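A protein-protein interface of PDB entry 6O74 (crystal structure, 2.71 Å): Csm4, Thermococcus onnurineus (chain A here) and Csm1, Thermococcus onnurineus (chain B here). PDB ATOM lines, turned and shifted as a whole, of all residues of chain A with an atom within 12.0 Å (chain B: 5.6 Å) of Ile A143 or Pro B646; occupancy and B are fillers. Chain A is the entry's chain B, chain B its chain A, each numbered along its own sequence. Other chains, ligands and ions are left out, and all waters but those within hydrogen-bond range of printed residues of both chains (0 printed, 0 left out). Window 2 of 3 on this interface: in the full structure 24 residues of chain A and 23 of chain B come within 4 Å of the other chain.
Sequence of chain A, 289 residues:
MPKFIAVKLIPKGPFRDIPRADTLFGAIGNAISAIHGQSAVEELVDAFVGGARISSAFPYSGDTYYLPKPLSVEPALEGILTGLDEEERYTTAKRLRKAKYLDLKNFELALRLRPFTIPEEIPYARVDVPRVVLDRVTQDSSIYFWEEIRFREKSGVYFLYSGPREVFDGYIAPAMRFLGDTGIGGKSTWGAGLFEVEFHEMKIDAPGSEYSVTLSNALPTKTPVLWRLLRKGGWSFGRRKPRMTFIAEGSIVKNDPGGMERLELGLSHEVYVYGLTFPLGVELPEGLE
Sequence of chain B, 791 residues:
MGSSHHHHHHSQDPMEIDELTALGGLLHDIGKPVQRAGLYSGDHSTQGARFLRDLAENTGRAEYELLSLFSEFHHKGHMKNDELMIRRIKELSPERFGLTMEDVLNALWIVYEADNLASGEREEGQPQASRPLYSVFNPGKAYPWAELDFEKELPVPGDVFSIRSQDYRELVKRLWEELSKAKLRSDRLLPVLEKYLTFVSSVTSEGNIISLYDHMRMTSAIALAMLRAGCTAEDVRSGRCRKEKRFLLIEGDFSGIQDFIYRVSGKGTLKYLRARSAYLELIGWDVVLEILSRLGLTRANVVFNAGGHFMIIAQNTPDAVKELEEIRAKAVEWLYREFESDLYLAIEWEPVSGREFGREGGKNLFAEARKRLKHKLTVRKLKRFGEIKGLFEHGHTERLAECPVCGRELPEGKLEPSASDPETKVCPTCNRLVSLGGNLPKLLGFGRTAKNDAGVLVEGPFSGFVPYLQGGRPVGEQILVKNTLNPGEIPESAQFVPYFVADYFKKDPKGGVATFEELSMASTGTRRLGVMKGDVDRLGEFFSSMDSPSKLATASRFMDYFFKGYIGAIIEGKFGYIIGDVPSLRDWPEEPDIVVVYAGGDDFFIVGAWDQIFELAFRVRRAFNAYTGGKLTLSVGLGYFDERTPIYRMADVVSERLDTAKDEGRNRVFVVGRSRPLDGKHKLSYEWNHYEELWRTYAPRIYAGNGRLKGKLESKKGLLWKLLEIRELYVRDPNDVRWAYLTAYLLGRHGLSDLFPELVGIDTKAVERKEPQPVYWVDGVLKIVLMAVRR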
ATOM      1  N   ASP A 128       3.623  -3.924  21.174  1.00  0.00           N
ATOM      2  CA  ASP A 128       2.397  -4.761  21.057  1.00  0.00           C
ATOM      3  C   ASP A 128       2.759  -6.214  21.405  1.00  0.00           C
ATOM      4  O   ASP A 128       3.630  -6.794  20.731  1.00  0.00           O
ATOM      5  CB  ASP A 128       1.674  -4.576  19.716  1.00  0.00           C
ATOM      6  CG  ASP A 128       2.528  -4.629  18.463  1.00  0.00           C
ATOM      7  OD1 ASP A 128       3.655  -5.154  18.530  1.00  0.00           O
ATOM      8  OD2 ASP A 128       2.045  -4.143  17.423  1.00  0.00           O
ATOM      9  N   VAL A 129       2.106  -6.764  22.435  1.00  0.00           N
ATOM     10  CA  VAL A 129       2.442  -8.085  23.044  1.00  0.00           C
ATOM     11  C   VAL A 129       1.550  -9.143  22.406  1.00  0.00           C
ATOM     12  O   VAL A 129       0.335  -8.950  22.309  1.00  0.00           O
ATOM     13  CB  VAL A 129       2.275  -8.060  24.575  1.00  0.00           C
ATOM     14  CG1 VAL A 129       2.985  -9.239  25.229  1.00  0.00           C
ATOM     15  CG2 VAL A 129       2.754  -6.741  25.168  1.00  0.00           C
ATOM     16  N   PRO A 130       2.124 -10.283  21.955  1.00  0.00           N
ATOM     17  CA  PRO A 130       1.347 -11.350  21.336  1.00  0.00           C
ATOM     18  C   PRO A 130       0.863 -12.340  22.400  1.00  0.00           C
ATOM     19  O   PRO A 130       1.565 -12.546  23.372  1.00  0.00           O
ATOM     20  CB  PRO A 130       2.386 -12.017  20.430  1.00  0.00           C
ATOM     21  CG  PRO A 130       3.657 -11.938  21.256  1.00  0.00           C
ATOM     22  CD  PRO A 130       3.551 -10.639  22.036  1.00  0.00           C
ATOM     23  N   ARG A 131      -0.307 -12.931  22.190  1.00  0.00           N
ATOM     24  CA  ARG A 131      -0.802 -14.053  23.020  1.00  0.00           C
ATOM     25  C   ARG A 131      -1.525 -15.036  22.097  1.00  0.00           C
ATOM     26  O   ARG A 131      -2.174 -14.574  21.133  1.00  0.00           O
ATOM     27  CB  ARG A 131      -1.657 -13.517  24.173  1.00  0.00           C
ATOM     28  CG  ARG A 131      -0.915 -12.537  25.071  1.00  0.00           C
ATOM     29  CD  ARG A 131      -1.560 -12.333  26.429  1.00  0.00           C
ATOM     30  NE  ARG A 131      -0.653 -11.693  27.377  1.00  0.00           N
ATOM     31  CZ  ARG A 131      -0.910 -11.513  28.673  1.00  0.00           C
ATOM     32  NH1 ARG A 131      -2.057 -11.921  29.192  1.00  0.00           N
ATOM     33  NH2 ARG A 131      -0.013 -10.922  29.448  1.00  0.00           N
ATOM     34  N   VAL A 132      -1.357 -16.337  22.363  1.00  0.00           N
ATOM     35  CA  VAL A 132      -2.036 -17.447  21.631  1.00  0.00           C
ATOM     36  C   VAL A 132      -3.463 -17.564  22.184  1.00  0.00           C
ATOM     37  O   VAL A 132      -3.629 -17.378  23.401  1.00  0.00           O
ATOM     38  CB  VAL A 132      -1.258 -18.775  21.756  1.00  0.00           C
ATOM     39  CG1 VAL A 132      -1.873 -19.870  20.896  1.00  0.00           C
ATOM     40  CG2 VAL A 132       0.214 -18.609  21.412  1.00  0.00           C
ATOM     41  N   VAL A 133      -4.448 -17.853  21.325  1.00  0.00           N
ATOM     42  CA  VAL A 133      -5.895 -17.938  21.694  1.00  0.00           C
ATOM     43  C   VAL A 133      -6.447 -19.317  21.300  1.00  0.00           C
ATOM     44  O   VAL A 133      -6.258 -19.706  20.131  1.00  0.00           O
ATOM     45  CB  VAL A 133      -6.696 -16.796  21.035  1.00  0.00           C
ATOM     46  CG1 VAL A 133      -8.199 -16.991  21.176  1.00  0.00           C
ATOM     47  CG2 VAL A 133      -6.277 -15.439  21.581  1.00  0.00           C
ATOM     48  N   LEU A 134      -7.120 -20.002  22.237  1.00  0.00           N
ATOM     49  CA  LEU A 134      -7.785 -21.324  22.049  1.00  0.00           C
ATOM     50  C   LEU A 134      -6.801 -22.316  21.411  1.00  0.00           C
ATOM     51  O   LEU A 134      -6.151 -23.054  22.179  1.00  0.00           O
ATOM     52  CB  LEU A 134      -9.036 -21.138  21.180  1.00  0.00           C
ATOM     53  CG  LEU A 134      -9.915 -22.378  20.982  1.00  0.00           C
ATOM     54  CD1 LEU A 134     -10.560 -22.824  22.288  1.00  0.00           C
ATOM     55  CD2 LEU A 134     -10.987 -22.121  19.929  1.00  0.00           C
ATOM     56  N   SER A 141      -6.053 -22.578  17.246  1.00  0.00           N
ATOM     57  CA  SER A 141      -5.132 -21.641  17.952  1.00  0.00           C
ATOM     58  C   SER A 141      -4.630 -20.563  16.977  1.00  0.00           C
ATOM     59  O   SER A 141      -4.433 -20.888  15.791  1.00  0.00           O
ATOM     60  CB  SER A 141      -3.977 -22.376  18.604  1.00  0.00           C
ATOM     61  OG  SER A 141      -2.987 -22.725  17.648  1.00  0.00           O
ATOM     62  N   SER A 142      -4.437 -19.327  17.457  1.00  0.00           N
ATOM     63  CA  SER A 142      -3.930 -18.176  16.657  1.00  0.00           C
ATOM     64  C   SER A 142      -3.192 -17.174  17.556  1.00  0.00           C
ATOM     65  O   SER A 142      -3.303 -17.289  18.799  1.00  0.00           O
ATOM     66  CB  SER A 142      -5.047 -17.504  15.882  1.00  0.00           C
ATOM     67  OG  SER A 142      -5.931 -16.801  16.747  1.00  0.00           O
ATOM     68  N   ILE A 143      -2.470 -16.228  16.940  1.00  0.00           N
ATOM     69  CA  ILE A 143      -1.727 -15.136  17.646  1.00  0.00           C
ATOM     70  C   ILE A 143      -2.512 -13.826  17.481  1.00  0.00           C
ATOM     71  O   ILE A 143      -2.798 -13.441  16.329  1.00  0.00           O
ATOM     72  CB  ILE A 143      -0.276 -14.993  17.131  1.00  0.00           C
ATOM     73  CG1 ILE A 143       0.406 -16.345  16.879  1.00  0.00           C
ATOM     74  CG2 ILE A 143       0.523 -14.098  18.072  1.00  0.00           C
ATOM     75  CD1 ILE A 143       1.566 -16.676  17.801  1.00  0.00           C
ATOM     76  N   TYR A 144      -2.858 -13.177  18.596  1.00  0.00           N
ATOM     77  CA  TYR A 144      -3.497 -11.834  18.643  1.00  0.00           C
ATOM     78  C   TYR A 144      -2.531 -10.882  19.347  1.00  0.00           C
ATOM     79  O   TYR A 144      -1.680 -11.362  20.118  1.00  0.00           O
ATOM     80  CB  TYR A 144      -4.889 -11.909  19.283  1.00  0.00           C
ATOM     81  CG  TYR A 144      -5.985 -12.247  18.302  1.00  0.00           C
ATOM     82  CD1 TYR A 144      -6.713 -11.248  17.673  1.00  0.00           C
ATOM     83  CD2 TYR A 144      -6.270 -13.566  17.967  1.00  0.00           C
ATOM     84  CE1 TYR A 144      -7.706 -11.547  16.753  1.00  0.00           C
ATOM     85  CE2 TYR A 144      -7.259 -13.882  17.048  1.00  0.00           C
ATOM     86  CZ  TYR A 144      -7.979 -12.868  16.438  1.00  0.00           C
ATOM     87  OH  TYR A 144      -8.953 -13.176  15.532  1.00  0.00           O
ATOM     88  N   PHE A 145      -2.625  -9.588  19.036  1.00  0.00           N
ATOM     89  CA  PHE A 145      -1.697  -8.531  19.516  1.00  0.00           C
ATOM     90  C   PHE A 145      -2.490  -7.405  20.178  1.00  0.00           C
ATOM     91  O   PHE A 145      -3.428  -6.882  19.545  1.00  0.00           O
ATOM     92  CB  PHE A 145      -0.852  -7.983  18.365  1.00  0.00           C
ATOM     93  CG  PHE A 145       0.250  -8.905  17.921  1.00  0.00           C
ATOM     94  CD1 PHE A 145       1.527  -8.788  18.451  1.00  0.00           C
ATOM     95  CD2 PHE A 145       0.003  -9.899  16.986  1.00  0.00           C
ATOM     96  CE1 PHE A 145       2.543  -9.639  18.041  1.00  0.00           C
ATOM     97  CE2 PHE A 145       1.020 -10.753  16.582  1.00  0.00           C
ATOM     98  CZ  PHE A 145       2.286 -10.624  17.111  1.00  0.00           C
ATOM     99  N   TRP A 146      -2.103  -7.052  21.409  1.00  0.00           N
ATOM    100  CA  TRP A 146      -2.628  -5.883  22.162  1.00  0.00           C
ATOM    101  C   TRP A 146      -1.532  -4.825  22.233  1.00  0.00           C
ATOM    102  O   TRP A 146      -0.572  -5.005  23.009  1.00  0.00           O
ATOM    103  CB  TRP A 146      -3.133  -6.294  23.545  1.00  0.00           C
ATOM    104  CG  TRP A 146      -4.299  -7.225  23.453  1.00  0.00           C
ATOM    105  CD1 TRP A 146      -5.623  -6.904  23.521  1.00  0.00           C
ATOM    106  CD2 TRP A 146      -4.236  -8.638  23.195  1.00  0.00           C
ATOM    107  NE1 TRP A 146      -6.386  -8.027  23.351  1.00  0.00           N
ATOM    108  CE2 TRP A 146      -5.565  -9.107  23.150  1.00  0.00           C
ATOM    109  CE3 TRP A 146      -3.190  -9.549  23.016  1.00  0.00           C
ATOM    110  CZ2 TRP A 146      -5.871 -10.451  22.939  1.00  0.00           C
ATOM    111  CZ3 TRP A 146      -3.493 -10.875  22.805  1.00  0.00           C
ATOM    112  CH2 TRP A 146      -4.817 -11.318  22.768  1.00  0.00           C
ATOM    113  N   GLU A 147      -1.657  -3.810  21.378  1.00  0.00           N
ATOM    114  CA  GLU A 147      -0.831  -2.578  21.400  1.00  0.00           C
ATOM    115  C   GLU A 147      -0.872  -2.021  22.826  1.00  0.00           C
ATOM    116  O   GLU A 147      -1.976  -1.897  23.385  1.00  0.00           O
ATOM    117  CB  GLU A 147      -1.300  -1.568  20.346  1.00  0.00           C
ATOM    118  CG  GLU A 147      -2.815  -1.456  20.197  1.00  0.00           C
ATOM    119  CD  GLU A 147      -3.495  -2.528  19.354  1.00  0.00           C
ATOM    120  OE1 GLU A 147      -2.966  -2.862  18.270  1.00  0.00           O
ATOM    121  OE2 GLU A 147      -4.549  -3.039  19.789  1.00  0.00           O
ATOM    122  N   ASP B 642       6.497 -17.324  13.531  1.00  0.00           N
ATOM    123  CA  ASP B 642       5.477 -18.372  13.769  1.00  0.00           C
ATOM    124  C   ASP B 642       4.432 -18.243  12.664  1.00  0.00           C
ATOM    125  O   ASP B 642       3.973 -17.116  12.448  1.00  0.00           O
ATOM    126  CB  ASP B 642       4.869 -18.200  15.161  1.00  0.00           C
ATOM    127  CG  ASP B 642       3.823 -19.229  15.543  1.00  0.00           C
ATOM    128  OD1 ASP B 642       2.908 -19.486  14.727  1.00  0.00           O
ATOM    129  OD2 ASP B 642       3.927 -19.753  16.666  1.00  0.00           O
ATOM    130  N   ARG B 644       1.509 -18.669  12.464  1.00  0.00           N
ATOM    131  CA  ARG B 644       0.198 -18.163  12.961  1.00  0.00           C
ATOM    132  C   ARG B 644       0.184 -16.631  13.081  1.00  0.00           C
ATOM    133  O   ARG B 644      -0.914 -16.102  13.343  1.00  0.00           O
ATOM    134  CB  ARG B 644      -0.146 -18.806  14.310  1.00  0.00           C
ATOM    135  CG  ARG B 644      -0.254 -20.324  14.251  1.00  0.00           C
ATOM    136  CD  ARG B 644      -0.860 -20.924  15.499  1.00  0.00           C
ATOM    137  NE  ARG B 644      -0.171 -20.539  16.725  1.00  0.00           N
ATOM    138  CZ  ARG B 644       0.965 -21.067  17.163  1.00  0.00           C
ATOM    139  NH1 ARG B 644       1.583 -22.004  16.464  1.00  0.00           N
ATOM    140  NH2 ARG B 644       1.492 -20.650  18.300  1.00  0.00           N
ATOM    141  N   THR B 645       1.323 -15.940  12.907  1.00  0.00           N
ATOM    142  CA  THR B 645       1.401 -14.451  12.969  1.00  0.00           C
ATOM    143  C   THR B 645       0.544 -13.870  11.845  1.00  0.00           C
ATOM    144  O   THR B 645       0.656 -14.315  10.707  1.00  0.00           O
ATOM    145  CB  THR B 645       2.835 -13.918  12.869  1.00  0.00           C
ATOM    146  OG1 THR B 645       3.737 -14.738  13.610  1.00  0.00           O
ATOM    147  CG2 THR B 645       2.948 -12.492  13.359  1.00  0.00           C
ATOM    148  N   PRO B 646      -0.371 -12.909  12.125  1.00  0.00           N
ATOM    149  CA  PRO B 646      -1.143 -12.254  11.067  1.00  0.00           C
ATOM    150  C   PRO B 646      -0.278 -11.411  10.112  1.00  0.00           C
ATOM    151  O   PRO B 646       0.703 -10.840  10.543  1.00  0.00           O
ATOM    152  CB  PRO B 646      -2.165 -11.372  11.813  1.00  0.00           C
ATOM    153  CG  PRO B 646      -1.621 -11.225  13.220  1.00  0.00           C
ATOM    154  CD  PRO B 646      -0.754 -12.442  13.467  1.00  0.00           C
ATOM    155  N   ILE B 647      -0.677 -11.362   8.837  1.00  0.00           N
ATOM    156  CA  ILE B 647       0.045 -10.653   7.735  1.00  0.00           C
ATOM    157  C   ILE B 647       0.420  -9.240   8.204  1.00  0.00           C
ATOM    158  O   ILE B 647       1.603  -8.864   8.049  1.00  0.00           O
ATOM    159  CB  ILE B 647      -0.794 -10.629   6.439  1.00  0.00           C
ATOM    160  CG1 ILE B 647      -2.140  -9.939   6.664  1.00  0.00           C
ATOM    161  CG2 ILE B 647      -0.963 -12.030   5.871  1.00  0.00           C
ATOM    162  CD1 ILE B 647      -3.256 -10.435   5.786  1.00  0.00           C
ATOM    163  N   TYR B 648      -0.529  -8.503   8.791  1.00  0.00           N
ATOM    164  CA  TYR B 648      -0.386  -7.054   9.097  1.00  0.00           C
ATOM    165  C   TYR B 648       0.847  -6.869   9.993  1.00  0.00           C
ATOM    166  O   TYR B 648       1.547  -5.834   9.864  1.00  0.00           O
ATOM    167  CB  TYR B 648      -1.672  -6.465   9.703  1.00  0.00           C
ATOM    168  CG  TYR B 648      -1.759  -6.553  11.204  1.00  0.00           C
ATOM    169  CD1 TYR B 648      -1.007  -5.708  12.007  1.00  0.00           C
ATOM    170  CD2 TYR B 648      -2.558  -7.499  11.831  1.00  0.00           C
ATOM    171  CE1 TYR B 648      -1.044  -5.799  13.390  1.00  0.00           C
ATOM    172  CE2 TYR B 648      -2.611  -7.602  13.213  1.00  0.00           C
ATOM    173  CZ  TYR B 648      -1.851  -6.747  13.993  1.00  0.00           C
ATOM    174  OH  TYR B 648      -1.885  -6.813  15.352  1.00  0.00           O
ATOM    175  N   ARG B 649       1.124  -7.849  10.857  1.00  0.00           N
ATOM    176  CA  ARG B 649       2.229  -7.759  11.844  1.00  0.00           C
ATOM    177  C   ARG B 649       3.557  -8.093  11.165  1.00  0.00           C
ATOM    178  O   ARG B 649       4.554  -7.392  11.441  1.00  0.00           O
ATOM    179  CB  ARG B 649       1.976  -8.673  13.045  1.00  0.00           C
ATOM    180  CG  ARG B 649       2.559  -8.123  14.340  1.00  0.00           C
ATOM    181  CD  ARG B 649       3.853  -8.800  14.711  1.00  0.00           C
ATOM    182  NE  ARG B 649       4.704  -8.000  15.583  1.00  0.00           N
ATOM    183  CZ  ARG B 649       5.802  -8.463  16.177  1.00  0.00           C
ATOM    184  NH1 ARG B 649       6.181  -9.728  16.010  1.00  0.00           N
ATOM    185  NH2 ARG B 649       6.515  -7.658  16.942  1.00  0.00           N
ATOM    186  N   MET B 650       3.571  -9.136  10.331  1.00  0.00           N
ATOM    187  CA  MET B 650       4.774  -9.567   9.574  1.00  0.00           C
ATOM    188  C   MET B 650       5.178  -8.426   8.635  1.00  0.00           C
ATOM    189  O   MET B 650       6.353  -8.023   8.672  1.00  0.00           O
ATOM    190  CB  MET B 650       4.489 -10.832   8.764  1.00  0.00           C
ATOM    191  CG  MET B 650       4.225 -12.053   9.614  1.00  0.00           C
ATOM    192  SD  MET B 650       3.717 -13.407   8.555  1.00  0.00           S
ATOM    193  CE  MET B 650       3.862 -14.809   9.654  1.00  0.00           C
ATOM    194  N   ALA B 651       4.221  -7.907   7.858  1.00  0.00           N
ATOM    195  CA  ALA B 651       4.403  -6.744   6.962  1.00  0.00           C
ATOM    196  C   ALA B 651       5.067  -5.604   7.749  1.00  0.00           C
ATOM    197  O   ALA B 651       6.074  -5.050   7.280  1.00  0.00           O
ATOM    198  CB  ALA B 651       3.074  -6.334   6.376  1.00  0.00           C
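The guanidinium group (NH2) of Arg B644 is in salt-bridge range of the side-chain carboxylate (OD2) of Asp B642 (3.1 Å).
Among the printed residues, merely in contact across the chains: Phe A145 with Tyr B648 (3.4 Å), Phe A145 with Arg B649 (3.4 Å), Ser A141 with Arg B644 (3.5 Å), Ile A143 with Arg B644 (3.6 Å), Ile A143 with Pro B646 (3.7 Å), Val A132 with Arg B644 (3.9 Å) and Phe A145 with Pro B646 (3.96 Å).
Of chain B, only Arg B644 and Pro B646 come within 4 Å of Ile A143. Of chain A, only Ile A143 (3.7 Å) and Phe A145 (3.96 Å) come within 4 Å of Pro B646. No residue of chain A comes within 4 Å of Asp B642. Arg B644 touches three residues of chain A. No residue of chain A comes within 4 Å of Thr B645. No residue of chain A comes within 4 Å of Met B650. Printed residues of chain B within 4 Å of Ser A141: Arg B644 (3.5 Å). Printed residues of chain B within 4 Å of Phe A145: Pro B646 (3.96 Å), Tyr B648 (3.4 Å) and Arg B649 (3.4 Å). Printed residues of chain A within 4 Å of Arg B649: Phe A145 (3.4 Å). Of the printed residues of chain B, Val A132 touches Arg B644. The nearest printed residue of chain B that does not touch Phe A145 is Thr B645 (4.1 Å).
Among the printed residues, no Asp or Glu carboxylate lies within 4 Å of a Lys or Arg side-chain nitrogen of the other chain.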
